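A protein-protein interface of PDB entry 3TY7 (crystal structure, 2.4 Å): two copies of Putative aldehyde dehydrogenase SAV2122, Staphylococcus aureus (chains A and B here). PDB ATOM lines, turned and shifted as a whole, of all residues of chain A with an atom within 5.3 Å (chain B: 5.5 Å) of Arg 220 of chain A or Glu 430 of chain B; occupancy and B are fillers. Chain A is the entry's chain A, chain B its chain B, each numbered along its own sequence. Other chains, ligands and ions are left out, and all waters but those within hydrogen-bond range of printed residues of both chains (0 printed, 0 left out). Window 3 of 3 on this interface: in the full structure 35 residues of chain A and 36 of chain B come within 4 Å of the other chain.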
ATOM      1  N   TYR A  58     -18.135 -23.702  -7.965  1.00  0.00           N
ATOM      2  CA  TYR A  58     -17.026 -24.575  -7.539  1.00  0.00           C
ATOM      3  C   TYR A  58     -17.432 -25.758  -6.653  1.00  0.00           C
ATOM      4  O   TYR A  58     -16.880 -26.851  -6.783  1.00  0.00           O
ATOM      5  CB  TYR A  58     -15.858 -23.782  -6.924  1.00  0.00           C
ATOM      6  CG  TYR A  58     -15.883 -23.647  -5.417  1.00  0.00           C
ATOM      7  CD1 TYR A  58     -15.318 -24.620  -4.599  1.00  0.00           C
ATOM      8  CD2 TYR A  58     -16.442 -22.531  -4.813  1.00  0.00           C
ATOM      9  CE1 TYR A  58     -15.331 -24.494  -3.224  1.00  0.00           C
ATOM     10  CE2 TYR A  58     -16.456 -22.392  -3.440  1.00  0.00           C
ATOM     11  CZ  TYR A  58     -15.900 -23.376  -2.650  1.00  0.00           C
ATOM     12  OH  TYR A  58     -15.915 -23.241  -1.282  1.00  0.00           O
ATOM     13  N   LEU A  59     -18.378 -25.535  -5.747  1.00  0.00           N
ATOM     14  CA  LEU A  59     -18.889 -26.616  -4.913  1.00  0.00           C
ATOM     15  C   LEU A  59     -19.622 -27.643  -5.766  1.00  0.00           C
ATOM     16  O   LEU A  59     -19.505 -28.851  -5.553  1.00  0.00           O
ATOM     17  CB  LEU A  59     -19.823 -26.068  -3.835  1.00  0.00           C
ATOM     18  CG  LEU A  59     -19.135 -25.437  -2.624  1.00  0.00           C
ATOM     19  CD1 LEU A  59     -20.121 -24.627  -1.790  1.00  0.00           C
ATOM     20  CD2 LEU A  59     -18.466 -26.519  -1.784  1.00  0.00           C
ATOM     21  N   ARG A  62     -16.963 -29.601  -7.729  1.00  0.00           N
ATOM     22  CA  ARG A  62     -16.192 -30.447  -6.825  1.00  0.00           C
ATOM     23  C   ARG A  62     -16.919 -31.751  -6.527  1.00  0.00           C
ATOM     24  O   ARG A  62     -16.326 -32.831  -6.560  1.00  0.00           O
ATOM     25  CB  ARG A  62     -15.902 -29.710  -5.512  1.00  0.00           C
ATOM     26  CG  ARG A  62     -15.362 -30.609  -4.404  1.00  0.00           C
ATOM     27  CD  ARG A  62     -15.187 -29.845  -3.100  1.00  0.00           C
ATOM     28  NE  ARG A  62     -14.067 -28.912  -3.163  1.00  0.00           N
ATOM     29  CZ  ARG A  62     -13.875 -27.915  -2.305  1.00  0.00           C
ATOM     30  NH1 ARG A  62     -14.738 -27.711  -1.317  1.00  0.00           N
ATOM     31  NH2 ARG A  62     -12.826 -27.115  -2.442  1.00  0.00           N
ATOM     32  N   ILE A 140      -9.530 -28.522  -5.331  1.00  0.00           N
ATOM     33  CA  ILE A 140      -9.089 -27.399  -4.518  1.00  0.00           C
ATOM     34  C   ILE A 140      -9.996 -26.179  -4.725  1.00  0.00           C
ATOM     35  O   ILE A 140     -10.006 -25.261  -3.909  1.00  0.00           O
ATOM     36  CB  ILE A 140      -7.619 -27.041  -4.823  1.00  0.00           C
ATOM     37  CG1 ILE A 140      -7.059 -26.081  -3.771  1.00  0.00           C
ATOM     38  CG2 ILE A 140      -7.493 -26.468  -6.229  1.00  0.00           C
ATOM     39  CD1 ILE A 140      -5.583 -25.782  -3.929  1.00  0.00           C
ATOM     40  N   GLY A 141     -10.806 -26.198  -5.780  1.00  0.00           N
ATOM     41  CA  GLY A 141     -11.662 -25.064  -6.078  1.00  0.00           C
ATOM     42  C   GLY A 141     -11.101 -24.154  -7.152  1.00  0.00           C
ATOM     43  O   GLY A 141     -10.273 -24.577  -7.960  1.00  0.00           O
ATOM     44  N   VAL A 142     -11.575 -22.911  -7.171  1.00  0.00           N
ATOM     45  CA  VAL A 142     -11.274 -21.975  -8.250  1.00  0.00           C
ATOM     46  C   VAL A 142      -9.775 -21.818  -8.497  1.00  0.00           C
ATOM     47  O   VAL A 142      -9.014 -21.507  -7.584  1.00  0.00           O
ATOM     48  CB  VAL A 142     -11.866 -20.587  -7.946  1.00  0.00           C
ATOM     49  CG1 VAL A 142     -11.545 -19.620  -9.072  1.00  0.00           C
ATOM     50  CG2 VAL A 142     -13.372 -20.686  -7.726  1.00  0.00           C
ATOM     51  N   SER A 143      -9.369 -22.015  -9.748  1.00  0.00           N
ATOM     52  CA  SER A 143      -7.959 -22.031 -10.106  1.00  0.00           C
ATOM     53  C   SER A 143      -7.654 -21.066 -11.241  1.00  0.00           C
ATOM     54  O   SER A 143      -8.326 -21.082 -12.272  1.00  0.00           O
ATOM     55  CB  SER A 143      -7.555 -23.446 -10.522  1.00  0.00           C
ATOM     56  OG  SER A 143      -7.811 -24.364  -9.476  1.00  0.00           O
ATOM     57  N   LYS A 218     -10.636 -14.911  -4.101  1.00  0.00           N
ATOM     58  CA  LYS A 218     -11.431 -16.119  -4.317  1.00  0.00           C
ATOM     59  C   LYS A 218     -10.784 -17.148  -5.248  1.00  0.00           C
ATOM     60  O   LYS A 218     -11.381 -18.181  -5.556  1.00  0.00           O
ATOM     61  CB  LYS A 218     -12.854 -15.772  -4.757  1.00  0.00           C
ATOM     62  CG  LYS A 218     -13.713 -15.256  -3.616  1.00  0.00           C
ATOM     63  CD  LYS A 218     -15.154 -15.055  -4.035  1.00  0.00           C
ATOM     64  CE  LYS A 218     -15.978 -14.500  -2.884  1.00  0.00           C
ATOM     65  NZ  LYS A 218     -17.366 -14.145  -3.296  1.00  0.00           N
ATOM     66  N   VAL A 219      -9.564 -16.864  -5.691  1.00  0.00           N
ATOM     67  CA  VAL A 219      -8.775 -17.857  -6.410  1.00  0.00           C
ATOM     68  C   VAL A 219      -7.931 -18.620  -5.394  1.00  0.00           C
ATOM     69  O   VAL A 219      -7.057 -18.044  -4.746  1.00  0.00           O
ATOM     70  CB  VAL A 219      -7.841 -17.193  -7.435  1.00  0.00           C
ATOM     71  CG1 VAL A 219      -6.852 -18.207  -7.982  1.00  0.00           C
ATOM     72  CG2 VAL A 219      -8.643 -16.552  -8.558  1.00  0.00           C
ATOM     73  N   ARG A 220      -8.206 -19.910  -5.236  1.00  0.00           N
ATOM     74  CA  ARG A 220      -7.503 -20.706  -4.232  1.00  0.00           C
ATOM     75  C   ARG A 220      -6.237 -21.362  -4.762  1.00  0.00           C
ATOM     76  O   ARG A 220      -5.417 -21.861  -3.991  1.00  0.00           O
ATOM     77  CB  ARG A 220      -8.438 -21.763  -3.642  1.00  0.00           C
ATOM     78  CG  ARG A 220      -9.649 -21.155  -2.972  1.00  0.00           C
ATOM     79  CD  ARG A 220     -10.548 -22.191  -2.335  1.00  0.00           C
ATOM     80  NE  ARG A 220     -11.664 -21.542  -1.653  1.00  0.00           N
ATOM     81  CZ  ARG A 220     -12.637 -22.185  -1.018  1.00  0.00           C
ATOM     82  NH1 ARG A 220     -12.641 -23.512  -0.973  1.00  0.00           N
ATOM     83  NH2 ARG A 220     -13.607 -21.499  -0.427  1.00  0.00           N
ATOM     84  N   MET A 221      -6.073 -21.349  -6.078  1.00  0.00           N
ATOM     85  CA  MET A 221      -4.942 -22.022  -6.694  1.00  0.00           C
ATOM     86  C   MET A 221      -4.444 -21.245  -7.906  1.00  0.00           C
ATOM     87  O   MET A 221      -5.233 -20.818  -8.748  1.00  0.00           O
ATOM     88  CB  MET A 221      -5.348 -23.446  -7.089  1.00  0.00           C
ATOM     89  CG  MET A 221      -4.215 -24.453  -7.084  1.00  0.00           C
ATOM     90  SD  MET A 221      -3.420 -24.688  -8.838  1.00  0.00           S
ATOM     91  CE  MET A 221      -1.629 -25.183  -8.256  1.00  0.00           C
ATOM     92  N   MET A 222      -3.130 -21.087  -8.005  1.00  0.00           N
ATOM     93  CA  MET A 222      -2.537 -20.360  -9.117  1.00  0.00           C
ATOM     94  C   MET A 222      -1.502 -21.226  -9.833  1.00  0.00           C
ATOM     95  O   MET A 222      -0.530 -21.675  -9.226  1.00  0.00           O
ATOM     96  CB  MET A 222      -1.892 -19.066  -8.613  1.00  0.00           C
ATOM     97  CG  MET A 222      -1.761 -17.984  -9.664  1.00  0.00           C
ATOM     98  SD  MET A 222      -3.483 -17.214 -10.160  1.00  0.00           S
ATOM     99  CE  MET A 222      -2.940 -16.401 -11.840  1.00  0.00           C
ATOM    100  N   ASP A 241      -2.254 -13.955  -0.323  1.00  0.00           N
ATOM    101  CA  ASP A 241      -3.520 -14.668  -0.248  1.00  0.00           C
ATOM    102  C   ASP A 241      -3.295 -16.125   0.144  1.00  0.00           C
ATOM    103  O   ASP A 241      -4.247 -16.864   0.405  1.00  0.00           O
ATOM    104  CB  ASP A 241      -4.226 -14.587  -1.602  1.00  0.00           C
ATOM    105  CG  ASP A 241      -5.644 -15.111  -1.554  1.00  0.00           C
ATOM    106  OD1 ASP A 241      -6.538 -14.356  -1.119  1.00  0.00           O
ATOM    107  OD2 ASP A 241      -5.864 -16.275  -1.954  1.00  0.00           O
ATOM    108  N   PHE A 242      -2.026 -16.521   0.192  1.00  0.00           N
ATOM    109  CA  PHE A 242      -1.632 -17.902   0.471  1.00  0.00           C
ATOM    110  C   PHE A 242      -2.239 -18.894  -0.518  1.00  0.00           C
ATOM    111  O   PHE A 242      -2.755 -19.942  -0.131  1.00  0.00           O
ATOM    112  CB  PHE A 242      -1.947 -18.293   1.919  1.00  0.00           C
ATOM    113  CG  PHE A 242      -1.147 -17.528   2.930  1.00  0.00           C
ATOM    114  CD1 PHE A 242       0.205 -17.778   3.088  1.00  0.00           C
ATOM    115  CD2 PHE A 242      -1.741 -16.555   3.718  1.00  0.00           C
ATOM    116  CE1 PHE A 242       0.951 -17.075   4.011  1.00  0.00           C
ATOM    117  CE2 PHE A 242      -0.999 -15.849   4.646  1.00  0.00           C
ATOM    118  CZ  PHE A 242       0.348 -16.110   4.790  1.00  0.00           C
ATOM    119  N   LYS A 243      -2.171 -18.541  -1.799  1.00  0.00           N
ATOM    120  CA  LYS A 243      -2.582 -19.430  -2.876  1.00  0.00           C
ATOM    121  C   LYS A 243      -1.524 -20.506  -3.085  1.00  0.00           C
ATOM    122  O   LYS A 243      -0.334 -20.273  -2.865  1.00  0.00           O
ATOM    123  CB  LYS A 243      -2.749 -18.649  -4.179  1.00  0.00           C
ATOM    124  CG  LYS A 243      -3.722 -17.490  -4.120  1.00  0.00           C
ATOM    125  CD  LYS A 243      -3.655 -16.699  -5.414  1.00  0.00           C
ATOM    126  CE  LYS A 243      -4.910 -15.881  -5.647  1.00  0.00           C
ATOM    127  NZ  LYS A 243      -5.056 -14.762  -4.684  1.00  0.00           N
ATOM    128  N   LYS A 244      -1.959 -21.684  -3.515  1.00  0.00           N
ATOM    129  CA  LYS A 244      -1.035 -22.739  -3.900  1.00  0.00           C
ATOM    130  C   LYS A 244      -0.445 -22.392  -5.265  1.00  0.00           C
ATOM    131  O   LYS A 244      -1.182 -22.153  -6.221  1.00  0.00           O
ATOM    132  CB  LYS A 244      -1.765 -24.082  -3.946  1.00  0.00           C
ATOM    133  CG  LYS A 244      -0.931 -25.248  -4.445  1.00  0.00           C
ATOM    134  CD  LYS A 244      -1.742 -26.534  -4.395  1.00  0.00           C
ATOM    135  CE  LYS A 244      -1.020 -27.687  -5.072  1.00  0.00           C
ATOM    136  NZ  LYS A 244      -1.828 -28.939  -5.016  1.00  0.00           N
ATOM    137  N   LYS A 471      -8.471 -34.596   2.382  1.00  0.00           N
ATOM    138  CA  LYS A 471      -9.144 -34.428   3.660  1.00  0.00           C
ATOM    139  C   LYS A 471      -9.262 -35.778   4.343  1.00  0.00           C
ATOM    140  O   LYS A 471      -9.688 -36.756   3.731  1.00  0.00           O
ATOM    141  CB  LYS A 471     -10.534 -33.809   3.475  1.00  0.00           C
ATOM    142  CG  LYS A 471     -11.466 -34.033   4.658  1.00  0.00           C
ATOM    143  CD  LYS A 471     -12.612 -33.032   4.697  1.00  0.00           C
ATOM    144  CE  LYS A 471     -13.524 -33.147   3.493  1.00  0.00           C
ATOM    145  NZ  LYS A 471     -14.685 -32.220   3.609  1.00  0.00           N
ATOM    146  N   ASN B 404     -18.312 -22.929   6.934  1.00  0.00           N
ATOM    147  CA  ASN B 404     -17.424 -22.755   5.796  1.00  0.00           C
ATOM    148  C   ASN B 404     -17.165 -21.305   5.420  1.00  0.00           C
ATOM    149  O   ASN B 404     -16.348 -21.042   4.536  1.00  0.00           O
ATOM    150  CB  ASN B 404     -17.931 -23.534   4.580  1.00  0.00           C
ATOM    151  CG  ASN B 404     -17.706 -25.024   4.712  1.00  0.00           C
ATOM    152  OD1 ASN B 404     -16.808 -25.466   5.431  1.00  0.00           O
ATOM    153  ND2 ASN B 404     -18.519 -25.807   4.015  1.00  0.00           N
ATOM    154  N   TYR B 408     -10.060 -19.651   6.667  1.00  0.00           N
ATOM    155  CA  TYR B 408      -9.202 -20.793   6.989  1.00  0.00           C
ATOM    156  C   TYR B 408      -9.787 -22.155   6.605  1.00  0.00           C
ATOM    157  O   TYR B 408     -10.981 -22.397   6.764  1.00  0.00           O
ATOM    158  CB  TYR B 408      -8.885 -20.805   8.480  1.00  0.00           C
ATOM    159  CG  TYR B 408      -8.325 -19.510   9.022  1.00  0.00           C
ATOM    160  CD1 TYR B 408      -6.996 -19.162   8.811  1.00  0.00           C
ATOM    161  CD2 TYR B 408      -9.115 -18.654   9.779  1.00  0.00           C
ATOM    162  CE1 TYR B 408      -6.475 -17.986   9.324  1.00  0.00           C
ATOM    163  CE2 TYR B 408      -8.606 -17.478  10.296  1.00  0.00           C
ATOM    164  CZ  TYR B 408      -7.286 -17.147  10.066  1.00  0.00           C
ATOM    165  OH  TYR B 408      -6.781 -15.974  10.581  1.00  0.00           O
ATOM    166  N   GLY B 409      -8.932 -23.032   6.087  1.00  0.00           N
ATOM    167  CA  GLY B 409      -9.306 -24.400   5.763  1.00  0.00           C
ATOM    168  C   GLY B 409      -8.754 -25.493   6.669  1.00  0.00           C
ATOM    169  O   GLY B 409      -8.672 -26.647   6.256  1.00  0.00           O
ATOM    170  N   LEU B 410      -8.322 -25.143   7.874  1.00  0.00           N
ATOM    171  CA  LEU B 410      -7.508 -26.069   8.667  1.00  0.00           C
ATOM    172  C   LEU B 410      -8.195 -27.306   9.276  1.00  0.00           C
ATOM    173  O   LEU B 410      -7.743 -28.432   9.068  1.00  0.00           O
ATOM    174  CB  LEU B 410      -6.745 -25.312   9.751  1.00  0.00           C
ATOM    175  CG  LEU B 410      -5.603 -26.118  10.362  1.00  0.00           C
ATOM    176  CD1 LEU B 410      -4.698 -26.673   9.276  1.00  0.00           C
ATOM    177  CD2 LEU B 410      -4.821 -25.243  11.295  1.00  0.00           C
ATOM    178  N   ALA B 411      -9.268 -27.099  10.029  1.00  0.00           N
ATOM    179  CA  ALA B 411      -9.901 -28.202  10.747  1.00  0.00           C
ATOM    180  C   ALA B 411     -11.393 -27.986  10.962  1.00  0.00           C
ATOM    181  O   ALA B 411     -11.900 -26.871  10.837  1.00  0.00           O
ATOM    182  CB  ALA B 411      -9.202 -28.445  12.083  1.00  0.00           C
ATOM    183  N   SER B 428     -19.246 -31.961   4.104  1.00  0.00           N
ATOM    184  CA  SER B 428     -19.558 -30.593   3.693  1.00  0.00           C
ATOM    185  C   SER B 428     -18.565 -29.550   4.202  1.00  0.00           C
ATOM    186  O   SER B 428     -18.273 -28.574   3.509  1.00  0.00           O
ATOM    187  CB  SER B 428     -20.978 -30.215   4.114  1.00  0.00           C
ATOM    188  OG  SER B 428     -21.935 -30.867   3.303  1.00  0.00           O
ATOM    189  N   ILE B 429     -18.070 -29.744   5.422  1.00  0.00           N
ATOM    190  CA  ILE B 429     -17.105 -28.823   6.011  1.00  0.00           C
ATOM    191  C   ILE B 429     -15.827 -28.809   5.188  1.00  0.00           C
ATOM    192  O   ILE B 429     -15.256 -29.862   4.911  1.00  0.00           O
ATOM    193  CB  ILE B 429     -16.743 -29.237   7.453  1.00  0.00           C
ATOM    194  CG1 ILE B 429     -17.979 -29.199   8.349  1.00  0.00           C
ATOM    195  CG2 ILE B 429     -15.649 -28.331   8.019  1.00  0.00           C
ATOM    196  CD1 ILE B 429     -17.697 -29.582   9.786  1.00  0.00           C
ATOM    197  N   GLU B 430     -15.353 -27.627   4.808  1.00  0.00           N
ATOM    198  CA  GLU B 430     -14.121 -27.591   4.046  1.00  0.00           C
ATOM    199  C   GLU B 430     -12.985 -27.434   5.035  1.00  0.00           C
ATOM    200  O   GLU B 430     -12.787 -26.367   5.614  1.00  0.00           O
ATOM    201  CB  GLU B 430     -14.122 -26.406   3.082  1.00  0.00           C
ATOM    202  CG  GLU B 430     -15.273 -26.397   2.089  1.00  0.00           C
ATOM    203  CD  GLU B 430     -15.261 -25.162   1.205  1.00  0.00           C
ATOM    204  OE1 GLU B 430     -15.416 -24.043   1.740  1.00  0.00           O
ATOM    205  OE2 GLU B 430     -15.085 -25.307  -0.022  1.00  0.00           O
ATOM    206  N   ALA B 431     -12.230 -28.512   5.205  1.00  0.00           N
ATOM    207  CA  ALA B 431     -11.075 -28.526   6.089  1.00  0.00           C
ATOM    208  C   ALA B 431     -10.170 -29.689   5.707  1.00  0.00           C
ATOM    209  O   ALA B 431     -10.619 -30.641   5.076  1.00  0.00           O
ATOM    210  CB  ALA B 431     -11.513 -28.642   7.536  1.00  0.00           C
ATOM    211  N   GLY B 432      -8.907 -29.629   6.109  1.00  0.00           N
ATOM    212  CA  GLY B 432      -7.990 -30.721   5.838  1.00  0.00           C
ATOM    213  C   GLY B 432      -8.236 -31.882   6.779  1.00  0.00           C
ATOM    214  O   GLY B 432      -7.952 -33.036   6.458  1.00  0.00           O
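The side-chain hydroxyl of Tyr 58 of chain A lies within hydrogen-bond range of the side-chain carboxylate of Glu 430 of chain B. OE2 of Glu 430 of chain B is in salt-bridge range of NH1 of Arg 62 of chain A, at 2.8 Å. The side-chain carboxylate of Glu 430 of chain B is in salt-bridge range of the guanidinium group of Arg 220 of chain A, 3.2 Å away. The side-chain amino group (NZ) of Lys 471 of chain A is in hydrogen-bond range of the backbone carbonyl oxygen (O) of Ile 429 of chain B, at 2.8 Å.
The side-chain hydroxyl of Tyr 58 of chain A sits at hydrogen-bond distance from the guanidinium group of Arg 220 of chain A, 3.0 Å away. The backbone carbonyl oxygen (O) of Val 142 of chain A lies within hydrogen-bond range of the backbone NH (N) of Arg 220 of chain A (3.0 Å). O of Arg 220 of chain A lies within hydrogen-bond range of N of Lys 244 of chain A (3.5 Å). OD1 of Asn 404 of chain B sits at hydrogen-bond distance from N of Glu 430 of chain B (2.7 Å). O of Gly 409 of chain B sits at hydrogen-bond distance from N of Gly 432 of chain B, at 3.0 Å. The backbone carbonyl oxygen (O) of Leu 410 of chain B sits at hydrogen-bond distance from the backbone NH (N) of Gly 432 of chain B (3.4 Å).
Among the printed residues, merely in contact across the chains: Lys 471 of chain A with Ala 431 of chain B and Lys 471 of chain A with Gly 432 of chain B.
Arg 220 of chain A touches just one residue of chain B: Glu 430. Printed residues of chain A within 4 Å of Glu 430 of chain B: Tyr 58 (2.6 Å), Arg 62 (2.8 Å) and Arg 220 (3.2 Å). Of the printed residues of chain B, Lys 471 of chain A touches Ile 429 (2.8 Å), Ala 431 (3.1 Å) and Gly 432 (3.3 Å). Of the printed residues of chain A, Ile 429 of chain B touches Lys 471 (2.8 Å). Of the printed residues of chain A, Gly 432 of chain B touches Lys 471 (3.3 Å). Gly 409 of chain B touches none of the printed residues of chain A. The nearest printed residue of chain A that does not touch Glu 430 of chain B is Leu 59 of chain A (4.001 Å). The nearest printed residue of chain A that does not touch Gly 432 of chain B is Arg 62 of chain A (9.6 Å).
Of the 10 printed residues of chain B, 4 touch a printed residue of chain A. Printed residues of chain B that touch a printed residue of chain A: Ile 429, Glu 430, Ala 431 and Gly 432. Hydrophobic or aromatic side chains of chain A within 4 Å of the printed part of chain B: Tyr 58. Among the printed residues, Asp or Glu carboxylates within 4 Å of a Lys or Arg side-chain nitrogen of the other chain: Arg 62 of chain A with Glu 430 of chain B (2.8 Å) and Arg 220 of chain A with Glu 430 of chain B (3.2 Å).
No position is printed for both chains.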
